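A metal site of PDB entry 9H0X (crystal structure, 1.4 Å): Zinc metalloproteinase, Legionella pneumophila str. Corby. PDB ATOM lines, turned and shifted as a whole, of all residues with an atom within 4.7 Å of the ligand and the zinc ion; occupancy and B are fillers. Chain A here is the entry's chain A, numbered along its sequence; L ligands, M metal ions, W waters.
Water W1 lies within hydrogen-bond range of OH of Tyr 185, NE2 of His 256 and N2 of the ligand.
Residues that only touch the ligand: Tyr 257, Leu 230 and Asp 254. Hydrophobic or aromatic side chains that line the ligand: His 170, His 174, Leu 230, His 256 and Tyr 257. 11 residues have an atom within 4 Å of the ligand: Asn 142, Ala 143, His 170, Glu 171, His 174, Glu 194, Leu 230, Arg 231, Asp 254, His 256 and Tyr 257.
A nitrogen (N1) of the ligand lies close to a ring nitrogen (NE2) of His 256, 3.5 Å away. OD1 of Asn 142 lies within hydrogen-bond range of N1 of the ligand (2.9 Å). The side-chain carboxylate (OE2) of Glu 171 lies within hydrogen-bond range of a nitrogen (N2) of the ligand, 2.9 Å away. NH1 of Arg 231 sits at hydrogen-bond distance from O4 of the ligand (2.8 Å). O of Ala 143 sits at hydrogen-bond distance from N2 of the ligand (2.7 Å).
The zinc ion is bound by NE2 of His 170 (2.0 Å), O1 of the ligand (2.1 Å), OE2 of Glu 194 (2.1 Å), NE2 of His 174 (2.1 Å) and O5 of the ligand (2.2 Å).
The nearest printed residue that does not touch the zinc ion is Tyr 185 (4.02 Å).
OE2 of Glu 194 sits close to NE2 of His 256, 3.3 Å away. NH2 of Arg 231 is in salt-bridge range of OE1 of Glu 194. OH of Tyr 140 sits at hydrogen-bond distance from ND2 of Asn 142 (3.2 Å). A ring nitrogen (ND1) of His 256 sits at hydrogen-bond distance from the side-chain carboxylate (OD2) of Asp 254 (2.7 Å). The side-chain carboxylate of Glu 194 sits close to the side-chain hydroxyl of Tyr 185. NE2 of His 256 lies within hydrogen-bond range of OH of Tyr 185, at 3.2 Å. N of Leu 230 is in hydrogen-bond range of O of Ile 216 (2.8 Å). N of Ile 216 lies within hydrogen-bond range of O of Arg 231.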
ATOM      1  N   TYR A 140      22.688 -27.428 -29.338  1.00  0.00           N
ATOM      2  CA  TYR A 140      22.417 -27.477 -27.877  1.00  0.00           C
ATOM      3  C   TYR A 140      23.610 -26.900 -27.129  1.00  0.00           C
ATOM      4  O   TYR A 140      24.670 -27.540 -27.113  1.00  0.00           O
ATOM      5  CB  TYR A 140      22.113 -28.928 -27.502  1.00  0.00           C
ATOM      6  CG  TYR A 140      21.628 -29.091 -26.070  1.00  0.00           C
ATOM      7  CD1 TYR A 140      20.346 -28.701 -25.711  1.00  0.00           C
ATOM      8  CD2 TYR A 140      22.437 -29.643 -25.090  1.00  0.00           C
ATOM      9  CE1 TYR A 140      19.892 -28.846 -24.415  1.00  0.00           C
ATOM     10  CE2 TYR A 140      21.990 -29.800 -23.793  1.00  0.00           C
ATOM     11  CZ  TYR A 140      20.717 -29.397 -23.450  1.00  0.00           C
ATOM     12  OH  TYR A 140      20.278 -29.543 -22.171  1.00  0.00           O
ATOM     13  N   GLU A 141      23.439 -25.749 -26.477  1.00  0.00           N
ATOM     14  CA  GLU A 141      24.556 -25.052 -25.788  1.00  0.00           C
ATOM     15  C   GLU A 141      24.503 -25.376 -24.286  1.00  0.00           C
ATOM     16  O   GLU A 141      24.379 -24.439 -23.485  1.00  0.00           O
ATOM     17  CB  GLU A 141      24.432 -23.559 -26.060  1.00  0.00           C
ATOM     18  CG  GLU A 141      24.452 -23.228 -27.538  1.00  0.00           C
ATOM     19  CD  GLU A 141      24.890 -21.806 -27.822  1.00  0.00           C
ATOM     20  OE1 GLU A 141      24.209 -20.854 -27.379  1.00  0.00           O
ATOM     21  OE2 GLU A 141      25.948 -21.664 -28.461  1.00  0.00           O
ATOM     22  N   ASN A 142      24.612 -26.654 -23.923  1.00  0.00           N
ATOM     23  CA  ASN A 142      24.564 -27.080 -22.532  1.00  0.00           C
ATOM     24  C   ASN A 142      25.086 -28.503 -22.459  1.00  0.00           C
ATOM     25  O   ASN A 142      25.330 -29.177 -23.476  1.00  0.00           O
ATOM     26  CB  ASN A 142      23.132 -26.971 -21.994  1.00  0.00           C
ATOM     27  CG  ASN A 142      23.026 -27.132 -20.498  1.00  0.00           C
ATOM     28  OD1 ASN A 142      23.841 -26.627 -19.757  1.00  0.00           O
ATOM     29  ND2 ASN A 142      22.030 -27.851 -20.060  1.00  0.00           N
ATOM     30  N   ALA A 143      25.253 -28.948 -21.218  1.00  0.00           N
ATOM     31  CA  ALA A 143      25.639 -30.318 -20.858  1.00  0.00           C
ATOM     32  C   ALA A 143      24.978 -30.596 -19.519  1.00  0.00           C
ATOM     33  O   ALA A 143      24.757 -29.662 -18.737  1.00  0.00           O
ATOM     34  CB  ALA A 143      27.161 -30.498 -20.772  1.00  0.00           C
ATOM     35  N   TYR A 144      24.690 -31.845 -19.213  1.00  0.00           N
ATOM     36  CA  TYR A 144      23.973 -32.146 -17.980  1.00  0.00           C
ATOM     37  C   TYR A 144      24.128 -33.606 -17.588  1.00  0.00           C
ATOM     38  O   TYR A 144      24.419 -34.486 -18.399  1.00  0.00           O
ATOM     39  CB  TYR A 144      22.483 -31.763 -18.104  1.00  0.00           C
ATOM     40  CG  TYR A 144      21.703 -32.501 -19.129  1.00  0.00           C
ATOM     41  CD1 TYR A 144      21.016 -33.696 -18.835  1.00  0.00           C
ATOM     42  CD2 TYR A 144      21.580 -32.021 -20.408  1.00  0.00           C
ATOM     43  CE1 TYR A 144      20.277 -34.360 -19.754  1.00  0.00           C
ATOM     44  CE2 TYR A 144      20.799 -32.720 -21.354  1.00  0.00           C
ATOM     45  CZ  TYR A 144      20.147 -33.877 -20.981  1.00  0.00           C
ATOM     46  OH  TYR A 144      19.407 -34.524 -22.007  1.00  0.00           O
ATOM     47  N   TRP A 145      23.830 -33.852 -16.306  1.00  0.00           N
ATOM     48  CA  TRP A 145      23.698 -35.178 -15.699  1.00  0.00           C
ATOM     49  C   TRP A 145      22.218 -35.481 -15.540  1.00  0.00           C
ATOM     50  O   TRP A 145      21.471 -34.639 -15.041  1.00  0.00           O
ATOM     51  CB  TRP A 145      24.401 -35.187 -14.323  1.00  0.00           C
ATOM     52  CG  TRP A 145      23.977 -36.291 -13.379  1.00  0.00           C
ATOM     53  CD1 TRP A 145      23.104 -36.150 -12.364  1.00  0.00           C
ATOM     54  CD2 TRP A 145      24.481 -37.628 -13.344  1.00  0.00           C
ATOM     55  NE1 TRP A 145      22.992 -37.345 -11.693  1.00  0.00           N
ATOM     56  CE2 TRP A 145      23.797 -38.275 -12.283  1.00  0.00           C
ATOM     57  CE3 TRP A 145      25.348 -38.376 -14.124  1.00  0.00           C
ATOM     58  CZ2 TRP A 145      24.013 -39.624 -11.960  1.00  0.00           C
ATOM     59  CZ3 TRP A 145      25.590 -39.744 -13.761  1.00  0.00           C
ATOM     60  CH2 TRP A 145      24.887 -40.321 -12.725  1.00  0.00           C
ATOM     61  N   LEU A 162      30.581 -29.000 -26.027  1.00  0.00           N
ATOM     62  CA  LEU A 162      30.783 -28.911 -24.574  1.00  0.00           C
ATOM     63  C   LEU A 162      31.486 -30.120 -24.035  1.00  0.00           C
ATOM     64  O   LEU A 162      31.017 -30.786 -23.124  1.00  0.00           O
ATOM     65  CB  LEU A 162      29.427 -28.720 -23.921  1.00  0.00           C
ATOM     66  CG  LEU A 162      28.750 -27.383 -24.050  1.00  0.00           C
ATOM     67  CD1 LEU A 162      29.673 -26.237 -23.695  1.00  0.00           C
ATOM     68  CD2 LEU A 162      28.183 -27.093 -25.337  1.00  0.00           C
ATOM     69  N   VAL A 167      34.468 -29.706 -18.231  1.00  0.00           N
ATOM     70  CA  VAL A 167      33.027 -29.949 -18.362  1.00  0.00           C
ATOM     71  C   VAL A 167      32.733 -31.404 -18.056  1.00  0.00           C
ATOM     72  O   VAL A 167      31.740 -31.737 -17.366  1.00  0.00           O
ATOM     73  CB  VAL A 167      32.478 -29.559 -19.764  1.00  0.00           C
ATOM     74  CG1 VAL A 167      31.006 -29.889 -19.859  1.00  0.00           C
ATOM     75  CG2 VAL A 167      32.635 -28.090 -20.020  1.00  0.00           C
ATOM     76  N   HIS A 170      32.847 -31.863 -14.316  1.00  0.00           N
ATOM     77  CA  HIS A 170      31.665 -31.261 -13.745  1.00  0.00           C
ATOM     78  C   HIS A 170      30.514 -32.236 -13.826  1.00  0.00           C
ATOM     79  O   HIS A 170      29.812 -32.488 -12.850  1.00  0.00           O
ATOM     80  CB  HIS A 170      31.361 -29.935 -14.476  1.00  0.00           C
ATOM     81  CG  HIS A 170      30.147 -29.242 -14.015  1.00  0.00           C
ATOM     82  ND1 HIS A 170      30.122 -28.063 -13.297  1.00  0.00           N
ATOM     83  CD2 HIS A 170      28.859 -29.576 -14.195  1.00  0.00           C
ATOM     84  CE1 HIS A 170      28.878 -27.727 -13.068  1.00  0.00           C
ATOM     85  NE2 HIS A 170      28.115 -28.658 -13.572  1.00  0.00           N
ATOM     86  N   GLU A 171      30.224 -32.742 -15.014  1.00  0.00           N
ATOM     87  CA  GLU A 171      29.007 -33.533 -15.186  1.00  0.00           C
ATOM     88  C   GLU A 171      29.089 -34.860 -14.456  1.00  0.00           C
ATOM     89  O   GLU A 171      28.118 -35.273 -13.817  1.00  0.00           O
ATOM     90  CB  GLU A 171      28.662 -33.775 -16.667  1.00  0.00           C
ATOM     91  CG  GLU A 171      28.467 -32.513 -17.460  1.00  0.00           C
ATOM     92  CD  GLU A 171      27.521 -31.521 -16.998  1.00  0.00           C
ATOM     93  OE1 GLU A 171      26.717 -31.744 -16.096  1.00  0.00           O
ATOM     94  OE2 GLU A 171      27.700 -30.363 -17.494  1.00  0.00           O
ATOM     95  N   HIS A 174      28.285 -34.549 -10.779  1.00  0.00           N
ATOM     96  CA  HIS A 174      26.900 -34.530 -10.352  1.00  0.00           C
ATOM     97  C   HIS A 174      26.452 -35.909  -9.920  1.00  0.00           C
ATOM     98  O   HIS A 174      25.673 -36.065  -8.985  1.00  0.00           O
ATOM     99  CB  HIS A 174      25.988 -34.040 -11.472  1.00  0.00           C
ATOM    100  CG  HIS A 174      25.914 -32.561 -11.620  1.00  0.00           C
ATOM    101  ND1 HIS A 174      25.617 -31.694 -10.587  1.00  0.00           N
ATOM    102  CD2 HIS A 174      26.099 -31.793 -12.704  1.00  0.00           C
ATOM    103  CE1 HIS A 174      25.618 -30.458 -11.049  1.00  0.00           C
ATOM    104  NE2 HIS A 174      25.893 -30.487 -12.352  1.00  0.00           N
ATOM    105  N   TYR A 185      18.720 -30.730  -6.027  1.00  0.00           N
ATOM    106  CA  TYR A 185      19.039 -29.758  -7.100  1.00  0.00           C
ATOM    107  C   TYR A 185      18.141 -28.517  -7.108  1.00  0.00           C
ATOM    108  O   TYR A 185      17.593 -28.104  -8.149  1.00  0.00           O
ATOM    109  CB  TYR A 185      19.037 -30.477  -8.440  1.00  0.00           C
ATOM    110  CG  TYR A 185      19.874 -29.820  -9.474  1.00  0.00           C
ATOM    111  CD1 TYR A 185      21.223 -29.885  -9.372  1.00  0.00           C
ATOM    112  CD2 TYR A 185      19.317 -29.156 -10.556  1.00  0.00           C
ATOM    113  CE1 TYR A 185      22.060 -29.336 -10.365  1.00  0.00           C
ATOM    114  CE2 TYR A 185      20.121 -28.600 -11.524  1.00  0.00           C
ATOM    115  CZ  TYR A 185      21.473 -28.682 -11.426  1.00  0.00           C
ATOM    116  OH  TYR A 185      22.246 -28.097 -12.407  1.00  0.00           O
ATOM    117  N   GLU A 194      25.868 -27.727  -7.609  1.00  0.00           N
ATOM    118  CA  GLU A 194      26.540 -27.137  -8.756  1.00  0.00           C
ATOM    119  C   GLU A 194      27.962 -26.738  -8.450  1.00  0.00           C
ATOM    120  O   GLU A 194      28.889 -26.980  -9.242  1.00  0.00           O
ATOM    121  CB  GLU A 194      25.687 -25.931  -9.187  1.00  0.00           C
ATOM    122  CG  GLU A 194      24.725 -26.224 -10.300  1.00  0.00           C
ATOM    123  CD  GLU A 194      25.433 -26.717 -11.510  1.00  0.00           C
ATOM    124  OE1 GLU A 194      26.435 -26.156 -11.967  1.00  0.00           O
ATOM    125  OE2 GLU A 194      24.897 -27.694 -12.119  1.00  0.00           O
ATOM    126  N   ILE A 216      35.092 -21.635 -15.414  1.00  0.00           N
ATOM    127  CA  ILE A 216      34.320 -22.708 -15.997  1.00  0.00           C
ATOM    128  C   ILE A 216      34.009 -22.316 -17.413  1.00  0.00           C
ATOM    129  O   ILE A 216      33.458 -21.252 -17.671  1.00  0.00           O
ATOM    130  CB  ILE A 216      33.018 -22.997 -15.236  1.00  0.00           C
ATOM    131  CG1 ILE A 216      33.319 -23.362 -13.771  1.00  0.00           C
ATOM    132  CG2 ILE A 216      32.218 -24.058 -15.947  1.00  0.00           C
ATOM    133  CD1 ILE A 216      34.079 -24.666 -13.586  1.00  0.00           C
ATOM    134  N   LEU A 230      32.217 -18.978 -18.847  1.00  0.00           N
ATOM    135  CA  LEU A 230      30.837 -19.062 -18.372  1.00  0.00           C
ATOM    136  C   LEU A 230      30.730 -18.642 -16.924  1.00  0.00           C
ATOM    137  O   LEU A 230      29.836 -17.866 -16.569  1.00  0.00           O
ATOM    138  CB  LEU A 230      30.330 -20.492 -18.541  1.00  0.00           C
ATOM    139  CG  LEU A 230      28.867 -20.679 -18.223  1.00  0.00           C
ATOM    140  CD1 LEU A 230      27.944 -19.868 -19.153  1.00  0.00           C
ATOM    141  CD2 LEU A 230      28.533 -22.163 -18.300  1.00  0.00           C
ATOM    142  N   ARG A 231      31.611 -19.133 -16.060  1.00  0.00           N
ATOM    143  CA  ARG A 231      31.649 -18.754 -14.647  1.00  0.00           C
ATOM    144  C   ARG A 231      33.072 -18.488 -14.234  1.00  0.00           C
ATOM    145  O   ARG A 231      34.028 -19.051 -14.803  1.00  0.00           O
ATOM    146  CB  ARG A 231      31.076 -19.838 -13.725  1.00  0.00           C
ATOM    147  CG  ARG A 231      29.590 -19.999 -13.803  1.00  0.00           C
ATOM    148  CD  ARG A 231      29.039 -21.069 -12.850  1.00  0.00           C
ATOM    149  NE  ARG A 231      29.348 -22.421 -13.290  1.00  0.00           N
ATOM    150  CZ  ARG A 231      28.583 -23.119 -14.141  1.00  0.00           C
ATOM    151  NH1 ARG A 231      27.610 -22.571 -14.793  1.00  0.00           N
ATOM    152  NH2 ARG A 231      28.803 -24.423 -14.270  1.00  0.00           N
ATOM    153  N   ASP A 254      18.700 -19.221  -9.385  1.00  0.00           N
ATOM    154  CA  ASP A 254      19.025 -20.495 -10.015  1.00  0.00           C
ATOM    155  C   ASP A 254      20.312 -21.081  -9.428  1.00  0.00           C
ATOM    156  O   ASP A 254      21.265 -20.358  -9.101  1.00  0.00           O
ATOM    157  CB  ASP A 254      19.265 -20.292 -11.524  1.00  0.00           C
ATOM    158  CG  ASP A 254      19.473 -21.607 -12.267  1.00  0.00           C
ATOM    159  OD1 ASP A 254      18.455 -22.308 -12.440  1.00  0.00           O
ATOM    160  OD2 ASP A 254      20.560 -21.950 -12.662  1.00  0.00           O
ATOM    161  N   HIS A 256      22.797 -22.399 -10.837  1.00  0.00           N
ATOM    162  CA  HIS A 256      24.022 -22.054 -11.560  1.00  0.00           C
ATOM    163  C   HIS A 256      24.521 -20.643 -11.257  1.00  0.00           C
ATOM    164  O   HIS A 256      25.625 -20.297 -11.710  1.00  0.00           O
ATOM    165  CB  HIS A 256      23.785 -22.205 -13.072  1.00  0.00           C
ATOM    166  CG  HIS A 256      23.406 -23.568 -13.507  1.00  0.00           C
ATOM    167  ND1 HIS A 256      22.102 -23.949 -13.634  1.00  0.00           N
ATOM    168  CD2 HIS A 256      24.171 -24.612 -13.857  1.00  0.00           C
ATOM    169  CE1 HIS A 256      22.085 -25.211 -14.073  1.00  0.00           C
ATOM    170  NE2 HIS A 256      23.313 -25.632 -14.216  1.00  0.00           N
ATOM    171  N   TYR A 257      23.796 -19.918 -10.444  1.00  0.00           N
ATOM    172  CA  TYR A 257      24.172 -18.577  -9.972  1.00  0.00           C
ATOM    173  C   TYR A 257      24.440 -18.602  -8.486  1.00  0.00           C
ATOM    174  O   TYR A 257      25.393 -17.957  -7.986  1.00  0.00           O
ATOM    175  CB  TYR A 257      23.105 -17.547 -10.317  1.00  0.00           C
ATOM    176  CG  TYR A 257      22.738 -17.547 -11.787  1.00  0.00           C
ATOM    177  CD1 TYR A 257      23.659 -17.709 -12.765  1.00  0.00           C
ATOM    178  CD2 TYR A 257      21.431 -17.347 -12.166  1.00  0.00           C
ATOM    179  CE1 TYR A 257      23.298 -17.789 -14.159  1.00  0.00           C
ATOM    180  CE2 TYR A 257      21.054 -17.420 -13.551  1.00  0.00           C
ATOM    181  CZ  TYR A 257      22.004 -17.587 -14.472  1.00  0.00           C
ATOM    182  OH  TYR A 257      21.698 -17.646 -15.871  1.00  0.00           O
HETATM  183  C1  LIG L   1      22.938 -21.661 -16.545  1.00  0.00           C
HETATM  184  C2  LIG L   1      23.876 -22.649 -16.781  1.00  0.00           C
HETATM  185  C3  LIG L   1      23.460 -23.919 -17.180  1.00  0.00           C
HETATM  186  C4  LIG L   1      22.100 -24.175 -17.264  1.00  0.00           C
HETATM  187  C5  LIG L   1      21.178 -23.186 -16.979  1.00  0.00           C
HETATM  188  C6  LIG L   1      21.590 -21.922 -16.603  1.00  0.00           C
HETATM  189  C7  LIG L   1      26.165 -26.589 -17.320  1.00  0.00           C
HETATM  190  C8  LIG L   1      25.877 -27.466 -16.068  1.00  0.00           C
HETATM  191  C9  LIG L   1      20.584 -20.849 -16.248  1.00  0.00           C
HETATM  192  C10 LIG L   1      20.149 -19.946 -18.570  1.00  0.00           C
HETATM  193  C11 LIG L   1      19.009 -19.859 -19.311  1.00  0.00           C
HETATM  194  C12 LIG L   1      18.784 -19.357 -20.704  1.00  0.00           C
HETATM  195  C13 LIG L   1      27.674 -26.585 -17.608  1.00  0.00           C
HETATM  196  C14 LIG L   1      28.109 -25.773 -18.830  1.00  0.00           C
HETATM  197  C15 LIG L   1      27.558 -26.310 -20.135  1.00  0.00           C
HETATM  198  C16 LIG L   1      29.612 -25.689 -18.926  1.00  0.00           C
HETATM  199  C17 LIG L   1      19.044 -23.008 -21.272  1.00  0.00           C
HETATM  200  C18 LIG L   1      20.380 -23.477 -21.871  1.00  0.00           C
HETATM  201  C19 LIG L   1      21.341 -23.871 -20.762  1.00  0.00           C
HETATM  202  C20 LIG L   1      20.155 -24.615 -22.854  1.00  0.00           C
HETATM  203  C21 LIG L   1      25.609 -25.189 -17.057  1.00  0.00           C
HETATM  204  N1  LIG L   1      24.342 -24.968 -17.490  1.00  0.00           N
HETATM  205  N2  LIG L   1      25.614 -28.749 -16.311  1.00  0.00           N
HETATM  206  N3  LIG L   1      19.769 -20.488 -17.398  1.00  0.00           N
HETATM  207  N4  LIG L   1      18.456 -20.741 -17.400  1.00  0.00           N
HETATM  208  N5  LIG L   1      17.985 -20.363 -18.563  1.00  0.00           N
HETATM  209  N6  LIG L   1      19.185 -20.294 -21.759  1.00  0.00           N
HETATM  210  O1  LIG L   1      25.439 -29.607 -15.225  1.00  0.00           O
HETATM  211  O2  LIG L   1      16.998 -21.443 -21.558  1.00  0.00           O
HETATM  212  O3  LIG L   1      18.428 -21.846 -23.531  1.00  0.00           O
HETATM  213  O4  LIG L   1      26.249 -24.359 -16.406  1.00  0.00           O
HETATM  214  O5  LIG L   1      25.949 -27.025 -14.911  1.00  0.00           O
HETATM  215  S1  LIG L   1      18.291 -21.638 -22.120  1.00  0.00           S
HETATM  216 ZN    ZN M   1      26.072 -28.711 -13.482  1.00  0.00          ZN
HETATM  217  O   HOH W   1      22.795 -28.458 -15.082  1.00  0.00           O
